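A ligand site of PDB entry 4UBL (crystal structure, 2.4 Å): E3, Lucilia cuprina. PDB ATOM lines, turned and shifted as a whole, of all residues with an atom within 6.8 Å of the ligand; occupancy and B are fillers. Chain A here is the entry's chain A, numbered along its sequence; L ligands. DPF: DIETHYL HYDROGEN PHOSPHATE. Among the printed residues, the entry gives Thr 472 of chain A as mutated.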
ATOM      1  N   HIS A 134     -10.698  20.270 -18.420  1.00  0.00           N
ATOM      2  CA  HIS A 134     -10.763  20.417 -16.979  1.00  0.00           C
ATOM      3  C   HIS A 134     -12.143  20.031 -16.457  1.00  0.00           C
ATOM      4  O   HIS A 134     -13.134  20.021 -17.204  1.00  0.00           O
ATOM      5  CB  HIS A 134     -10.380  21.844 -16.555  1.00  0.00           C
ATOM      6  CG  HIS A 134     -11.386  22.876 -16.945  1.00  0.00           C
ATOM      7  ND1 HIS A 134     -12.484  23.179 -16.169  1.00  0.00           N
ATOM      8  CD2 HIS A 134     -11.463  23.678 -18.034  1.00  0.00           C
ATOM      9  CE1 HIS A 134     -13.199  24.121 -16.766  1.00  0.00           C
ATOM     10  NE2 HIS A 134     -12.602  24.432 -17.894  1.00  0.00           N
ATOM     11  N   GLY A 135     -12.186  19.666 -15.191  1.00  0.00           N
ATOM     12  CA  GLY A 135     -13.419  19.346 -14.513  1.00  0.00           C
ATOM     13  C   GLY A 135     -13.802  20.546 -13.689  1.00  0.00           C
ATOM     14  O   GLY A 135     -13.231  21.611 -13.852  1.00  0.00           O
ATOM     15  N   GLY A 136     -14.749  20.357 -12.780  1.00  0.00           N
ATOM     16  CA  GLY A 136     -15.287  21.469 -12.021  1.00  0.00           C
ATOM     17  C   GLY A 136     -16.799  21.528 -12.145  1.00  0.00           C
ATOM     18  O   GLY A 136     -17.375  22.615 -12.215  1.00  0.00           O
ATOM     19  N   GLY A 137     -17.425  20.363 -12.187  1.00  0.00           N
ATOM     20  CA  GLY A 137     -18.865  20.211 -12.265  1.00  0.00           C
ATOM     21  C   GLY A 137     -19.559  21.056 -13.325  1.00  0.00           C
ATOM     22  O   GLY A 137     -20.736  21.408 -13.155  1.00  0.00           O
ATOM     23  N   PHE A 138     -18.834  21.369 -14.396  1.00  0.00           N
ATOM     24  CA  PHE A 138     -19.307  22.304 -15.438  1.00  0.00           C
ATOM     25  C   PHE A 138     -19.633  23.707 -14.905  1.00  0.00           C
ATOM     26  O   PHE A 138     -20.235  24.517 -15.622  1.00  0.00           O
ATOM     27  CB  PHE A 138     -20.524  21.726 -16.175  1.00  0.00           C
ATOM     28  CG  PHE A 138     -20.305  20.344 -16.719  1.00  0.00           C
ATOM     29  CD1 PHE A 138     -19.589  20.138 -17.881  1.00  0.00           C
ATOM     30  CD2 PHE A 138     -20.837  19.224 -16.057  1.00  0.00           C
ATOM     31  CE1 PHE A 138     -19.385  18.865 -18.374  1.00  0.00           C
ATOM     32  CE2 PHE A 138     -20.634  17.961 -16.551  1.00  0.00           C
ATOM     33  CZ  PHE A 138     -19.912  17.776 -17.714  1.00  0.00           C
ATOM     34  N   ILE A 140     -17.145  25.448 -12.481  1.00  0.00           N
ATOM     35  CA  ILE A 140     -15.865  26.130 -12.254  1.00  0.00           C
ATOM     36  C   ILE A 140     -14.755  25.453 -13.056  1.00  0.00           C
ATOM     37  O   ILE A 140     -14.987  24.399 -13.651  1.00  0.00           O
ATOM     38  CB  ILE A 140     -15.437  26.161 -10.779  1.00  0.00           C
ATOM     39  CG1 ILE A 140     -15.204  24.728 -10.258  1.00  0.00           C
ATOM     40  CG2 ILE A 140     -16.432  26.959  -9.940  1.00  0.00           C
ATOM     41  CD1 ILE A 140     -14.593  24.660  -8.870  1.00  0.00           C
ATOM     42  N   GLU A 217     -10.570  14.905 -15.972  1.00  0.00           N
ATOM     43  CA  GLU A 217     -10.954  14.428 -14.641  1.00  0.00           C
ATOM     44  C   GLU A 217     -12.343  14.965 -14.221  1.00  0.00           C
ATOM     45  O   GLU A 217     -12.667  16.127 -14.489  1.00  0.00           O
ATOM     46  CB  GLU A 217      -9.893  14.836 -13.615  1.00  0.00           C
ATOM     47  CG  GLU A 217     -10.081  14.272 -12.212  1.00  0.00           C
ATOM     48  CD  GLU A 217     -10.661  15.284 -11.235  1.00  0.00           C
ATOM     49  OE1 GLU A 217     -10.491  16.513 -11.451  1.00  0.00           O
ATOM     50  OE2 GLU A 217     -11.289  14.837 -10.243  1.00  0.00           O
ATOM     51  N   SER A 218     -13.152  14.121 -13.587  1.00  0.00           N
ATOM     52  CA  SER A 218     -14.450  14.521 -13.014  1.00  0.00           C
ATOM     53  C   SER A 218     -15.417  14.983 -14.112  1.00  0.00           C
ATOM     54  O   SER A 218     -15.775  14.202 -14.980  1.00  0.00           O
ATOM     55  CB  SER A 218     -14.250  15.610 -11.965  1.00  0.00           C
ATOM     56  OG  SER A 218     -15.429  15.837 -11.210  1.00  0.00           O
ATOM     57  N   ALA A 219     -15.805  16.266 -14.103  1.00  0.00           N
ATOM     58  CA  ALA A 219     -16.632  16.813 -15.186  1.00  0.00           C
ATOM     59  C   ALA A 219     -15.873  16.787 -16.506  1.00  0.00           C
ATOM     60  O   ALA A 219     -16.472  16.735 -17.592  1.00  0.00           O
ATOM     61  CB  ALA A 219     -17.086  18.235 -14.872  1.00  0.00           C
ATOM     62  N   GLY A 220     -14.543  16.817 -16.426  1.00  0.00           N
ATOM     63  CA  GLY A 220     -13.712  16.753 -17.611  1.00  0.00           C
ATOM     64  C   GLY A 220     -13.762  15.365 -18.199  1.00  0.00           C
ATOM     65  O   GLY A 220     -13.682  15.199 -19.420  1.00  0.00           O
ATOM     66  N   SER A 244     -12.025   9.373 -13.125  1.00  0.00           N
ATOM     67  CA  SER A 244     -13.072   9.634 -12.122  1.00  0.00           C
ATOM     68  C   SER A 244     -14.317  10.279 -12.723  1.00  0.00           C
ATOM     69  O   SER A 244     -14.793  11.291 -12.229  1.00  0.00           O
ATOM     70  CB  SER A 244     -12.547  10.546 -10.981  1.00  0.00           C
ATOM     71  OG  SER A 244     -11.507   9.935 -10.229  1.00  0.00           O
ATOM     72  N   TRP A 251     -24.451  12.832 -11.720  1.00  0.00           N
ATOM     73  CA  TRP A 251     -24.211  14.296 -11.745  1.00  0.00           C
ATOM     74  C   TRP A 251     -23.870  14.877 -13.124  1.00  0.00           C
ATOM     75  O   TRP A 251     -23.625  16.078 -13.256  1.00  0.00           O
ATOM     76  CB  TRP A 251     -23.062  14.648 -10.767  1.00  0.00           C
ATOM     77  CG  TRP A 251     -21.851  13.744 -10.953  1.00  0.00           C
ATOM     78  CD1 TRP A 251     -21.597  12.569 -10.287  1.00  0.00           C
ATOM     79  CD2 TRP A 251     -20.782  13.914 -11.904  1.00  0.00           C
ATOM     80  NE1 TRP A 251     -20.424  12.014 -10.755  1.00  0.00           N
ATOM     81  CE2 TRP A 251     -19.908  12.808 -11.742  1.00  0.00           C
ATOM     82  CE3 TRP A 251     -20.467  14.885 -12.853  1.00  0.00           C
ATOM     83  CZ2 TRP A 251     -18.746  12.669 -12.506  1.00  0.00           C
ATOM     84  CZ3 TRP A 251     -19.314  14.744 -13.607  1.00  0.00           C
ATOM     85  CH2 TRP A 251     -18.468  13.633 -13.432  1.00  0.00           C
ATOM     86  N   MET A 308     -27.156  17.679  -8.221  1.00  0.00           N
ATOM     87  CA  MET A 308     -25.986  18.391  -7.723  1.00  0.00           C
ATOM     88  C   MET A 308     -25.823  19.772  -8.353  1.00  0.00           C
ATOM     89  O   MET A 308     -25.329  20.700  -7.701  1.00  0.00           O
ATOM     90  CB  MET A 308     -24.737  17.525  -7.973  1.00  0.00           C
ATOM     91  CG  MET A 308     -23.459  18.114  -7.424  1.00  0.00           C
ATOM     92  SD  MET A 308     -22.047  16.971  -7.555  1.00  0.00           S
ATOM     93  CE  MET A 308     -22.465  15.778  -6.290  1.00  0.00           C
ATOM     94  N   PHE A 309     -26.247  19.903  -9.599  1.00  0.00           N
ATOM     95  CA  PHE A 309     -26.060  21.136 -10.359  1.00  0.00           C
ATOM     96  C   PHE A 309     -27.346  21.531 -11.094  1.00  0.00           C
ATOM     97  O   PHE A 309     -27.997  20.697 -11.721  1.00  0.00           O
ATOM     98  CB  PHE A 309     -24.909  20.985 -11.354  1.00  0.00           C
ATOM     99  CG  PHE A 309     -23.585  20.607 -10.714  1.00  0.00           C
ATOM    100  CD1 PHE A 309     -22.931  21.492  -9.867  1.00  0.00           C
ATOM    101  CD2 PHE A 309     -22.996  19.371 -10.975  1.00  0.00           C
ATOM    102  CE1 PHE A 309     -21.708  21.147  -9.268  1.00  0.00           C
ATOM    103  CE2 PHE A 309     -21.762  19.018 -10.386  1.00  0.00           C
ATOM    104  CZ  PHE A 309     -21.131  19.919  -9.527  1.00  0.00           C
ATOM    105  N   PHE A 354     -13.714  13.332  -0.749  1.00  0.00           N
ATOM    106  CA  PHE A 354     -13.968  14.690  -1.206  1.00  0.00           C
ATOM    107  C   PHE A 354     -15.073  15.398  -0.405  1.00  0.00           C
ATOM    108  O   PHE A 354     -15.044  16.611  -0.225  1.00  0.00           O
ATOM    109  CB  PHE A 354     -14.355  14.656  -2.685  1.00  0.00           C
ATOM    110  CG  PHE A 354     -14.451  16.011  -3.299  1.00  0.00           C
ATOM    111  CD1 PHE A 354     -15.675  16.659  -3.380  1.00  0.00           C
ATOM    112  CD2 PHE A 354     -13.326  16.657  -3.760  1.00  0.00           C
ATOM    113  CE1 PHE A 354     -15.769  17.923  -3.932  1.00  0.00           C
ATOM    114  CE2 PHE A 354     -13.410  17.922  -4.313  1.00  0.00           C
ATOM    115  CZ  PHE A 354     -14.640  18.549  -4.393  1.00  0.00           C
ATOM    116  N   PHE A 355     -16.053  14.635   0.084  1.00  0.00           N
ATOM    117  CA  PHE A 355     -17.234  15.208   0.713  1.00  0.00           C
ATOM    118  C   PHE A 355     -17.092  15.484   2.202  1.00  0.00           C
ATOM    119  O   PHE A 355     -18.096  15.722   2.880  1.00  0.00           O
ATOM    120  CB  PHE A 355     -18.442  14.286   0.473  1.00  0.00           C
ATOM    121  CG  PHE A 355     -18.776  14.139  -0.979  1.00  0.00           C
ATOM    122  CD1 PHE A 355     -19.664  15.010  -1.589  1.00  0.00           C
ATOM    123  CD2 PHE A 355     -18.161  13.163  -1.748  1.00  0.00           C
ATOM    124  CE1 PHE A 355     -19.961  14.890  -2.925  1.00  0.00           C
ATOM    125  CE2 PHE A 355     -18.447  13.034  -3.095  1.00  0.00           C
ATOM    126  CZ  PHE A 355     -19.352  13.892  -3.693  1.00  0.00           C
ATOM    127  N   TYR A 420     -21.407   8.076  -6.812  1.00  0.00           N
ATOM    128  CA  TYR A 420     -20.974   9.058  -7.793  1.00  0.00           C
ATOM    129  C   TYR A 420     -19.941   8.531  -8.791  1.00  0.00           C
ATOM    130  O   TYR A 420     -19.800   9.086  -9.868  1.00  0.00           O
ATOM    131  CB  TYR A 420     -20.418  10.301  -7.082  1.00  0.00           C
ATOM    132  CG  TYR A 420     -21.477  11.078  -6.317  1.00  0.00           C
ATOM    133  CD1 TYR A 420     -22.492  11.764  -6.992  1.00  0.00           C
ATOM    134  CD2 TYR A 420     -21.469  11.127  -4.932  1.00  0.00           C
ATOM    135  CE1 TYR A 420     -23.485  12.471  -6.292  1.00  0.00           C
ATOM    136  CE2 TYR A 420     -22.450  11.826  -4.223  1.00  0.00           C
ATOM    137  CZ  TYR A 420     -23.453  12.494  -4.919  1.00  0.00           C
ATOM    138  OH  TYR A 420     -24.415  13.197  -4.222  1.00  0.00           O
ATOM    139  N   PHE A 421     -19.229   7.447  -8.473  1.00  0.00           N
ATOM    140  CA  PHE A 421     -18.134   7.042  -9.358  1.00  0.00           C
ATOM    141  C   PHE A 421     -18.042   5.557  -9.726  1.00  0.00           C
ATOM    142  O   PHE A 421     -18.028   5.207 -10.908  1.00  0.00           O
ATOM    143  CB  PHE A 421     -16.797   7.499  -8.751  1.00  0.00           C
ATOM    144  CG  PHE A 421     -16.700   8.988  -8.532  1.00  0.00           C
ATOM    145  CD1 PHE A 421     -16.500   9.848  -9.609  1.00  0.00           C
ATOM    146  CD2 PHE A 421     -16.809   9.524  -7.253  1.00  0.00           C
ATOM    147  CE1 PHE A 421     -16.412  11.203  -9.407  1.00  0.00           C
ATOM    148  CE2 PHE A 421     -16.713  10.891  -7.051  1.00  0.00           C
ATOM    149  CZ  PHE A 421     -16.519  11.730  -8.128  1.00  0.00           C
ATOM    150  N   TYR A 457      -7.835  22.153  -5.092  1.00  0.00           N
ATOM    151  CA  TYR A 457      -9.031  21.414  -4.683  1.00  0.00           C
ATOM    152  C   TYR A 457      -8.980  20.902  -3.243  1.00  0.00           C
ATOM    153  O   TYR A 457     -10.026  20.706  -2.615  1.00  0.00           O
ATOM    154  CB  TYR A 457      -9.265  20.238  -5.617  1.00  0.00           C
ATOM    155  CG  TYR A 457      -9.922  20.562  -6.924  1.00  0.00           C
ATOM    156  CD1 TYR A 457     -11.284  20.841  -6.986  1.00  0.00           C
ATOM    157  CD2 TYR A 457      -9.194  20.560  -8.111  1.00  0.00           C
ATOM    158  CE1 TYR A 457     -11.903  21.120  -8.196  1.00  0.00           C
ATOM    159  CE2 TYR A 457      -9.804  20.842  -9.322  1.00  0.00           C
ATOM    160  CZ  TYR A 457     -11.154  21.123  -9.365  1.00  0.00           C
ATOM    161  OH  TYR A 457     -11.763  21.404 -10.565  1.00  0.00           O
ATOM    162  N   MET A 460     -10.666  23.372  -0.965  1.00  0.00           N
ATOM    163  CA  MET A 460     -12.116  23.442  -1.065  1.00  0.00           C
ATOM    164  C   MET A 460     -12.788  22.287  -0.329  1.00  0.00           C
ATOM    165  O   MET A 460     -13.781  22.476   0.378  1.00  0.00           O
ATOM    166  CB  MET A 460     -12.542  23.462  -2.531  1.00  0.00           C
ATOM    167  CG  MET A 460     -14.033  23.444  -2.777  1.00  0.00           C
ATOM    168  SD  MET A 460     -14.458  22.785  -4.404  1.00  0.00           S
ATOM    169  CE  MET A 460     -13.400  23.775  -5.446  1.00  0.00           C
ATOM    170  N   HIS A 471     -10.866  12.115  -4.395  1.00  0.00           N
ATOM    171  CA  HIS A 471     -11.164  12.655  -5.711  1.00  0.00           C
ATOM    172  C   HIS A 471     -10.319  13.931  -5.933  1.00  0.00           C
ATOM    173  O   HIS A 471     -10.236  14.776  -5.039  1.00  0.00           O
ATOM    174  CB  HIS A 471     -12.669  12.929  -5.789  1.00  0.00           C
ATOM    175  CG  HIS A 471     -13.124  13.421  -7.118  1.00  0.00           C
ATOM    176  ND1 HIS A 471     -13.107  12.624  -8.244  1.00  0.00           N
ATOM    177  CD2 HIS A 471     -13.598  14.617  -7.512  1.00  0.00           C
ATOM    178  CE1 HIS A 471     -13.567  13.317  -9.274  1.00  0.00           C
ATOM    179  NE2 HIS A 471     -13.861  14.534  -8.851  1.00  0.00           N
ATOM    180  N   THR A 472      -9.684  14.055  -7.112  1.00  0.00           N
ATOM    181  CA  THR A 472      -8.741  15.146  -7.492  1.00  0.00           C
ATOM    182  C   THR A 472      -7.348  15.135  -6.844  1.00  0.00           C
ATOM    183  O   THR A 472      -6.554  16.047  -7.096  1.00  0.00           O
ATOM    184  CB  THR A 472      -9.274  16.595  -7.210  1.00  0.00           C
ATOM    185  OG1 THR A 472      -9.216  16.896  -5.803  1.00  0.00           O
ATOM    186  CG2 THR A 472     -10.688  16.794  -7.738  1.00  0.00           C
HETATM  187  O4  DPF L   1     -16.056  18.176 -11.836  1.00  0.00           O
HETATM  188  P1  DPF L   1     -16.087  17.081 -10.812  1.00  0.00           P
HETATM  189  O3  DPF L   1     -17.688  16.799 -10.480  1.00  0.00           O
HETATM  190  C1  DPF L   1     -18.013  15.563  -9.988  1.00  0.00           C
HETATM  191  C4  DPF L   1     -19.053  15.764  -8.915  1.00  0.00           C
HETATM  192  O1  DPF L   1     -15.583  17.796  -9.415  1.00  0.00           O
HETATM  193  C2  DPF L   1     -14.245  18.000  -9.247  1.00  0.00           C
HETATM  194  C3  DPF L   1     -13.978  18.024  -7.766  1.00  0.00           C
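The side-chain hydroxyl (OG) of Ser 218 is covalently linked to a phosphorus (P1) of the ligand. The backbone NH (N) of Gly 137 is in hydrogen-bond range of an oxygen (O4) of the ligand, 2.6 Å away. O4 of the ligand lies within hydrogen-bond range of N of Gly 136, 2.7 Å away. N of Ala 219 is in hydrogen-bond range of O4 of the ligand (3.0 Å).
NE2 of His 471 lies within hydrogen-bond range of OG of Ser 218, at 3.1 Å. A ring nitrogen (NE2) of His 471 sits close to the side-chain carboxylate (OE2) of Glu 217 (2.9 Å). The indole nitrogen (NE1) of Trp 251 sits at hydrogen-bond distance from the backbone carbonyl oxygen (O) of Tyr 420, 3.1 Å away.
Gly 135 touches the ligand (C to O4, 3.8 Å). Trp 251 touches the ligand. Met 308 touches the ligand (SD to C4, 3.5 Å). Phe 354 touches the ligand (CZ to C3, 3.5 Å). Tyr 457 touches the ligand (CE1 to C3, 3.8 Å). His 471 touches the ligand. CG2 of Thr 472 touches C3 of the ligand, 3.5 Å away. Hydrophobic or aromatic side chains that line the ligand: Ala 219, Trp 251, Met 308, Phe 354, Tyr 457 and His 471. Within 4 Å of the ligand: Gly 135, Gly 136, Gly 137, Ser 218, Ala 219, Trp 251, Met 308, Phe 354, Tyr 457, His 471 and Thr 472. The nearest printed residue that does not touch the ligand is Glu 217 (4.4 Å).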
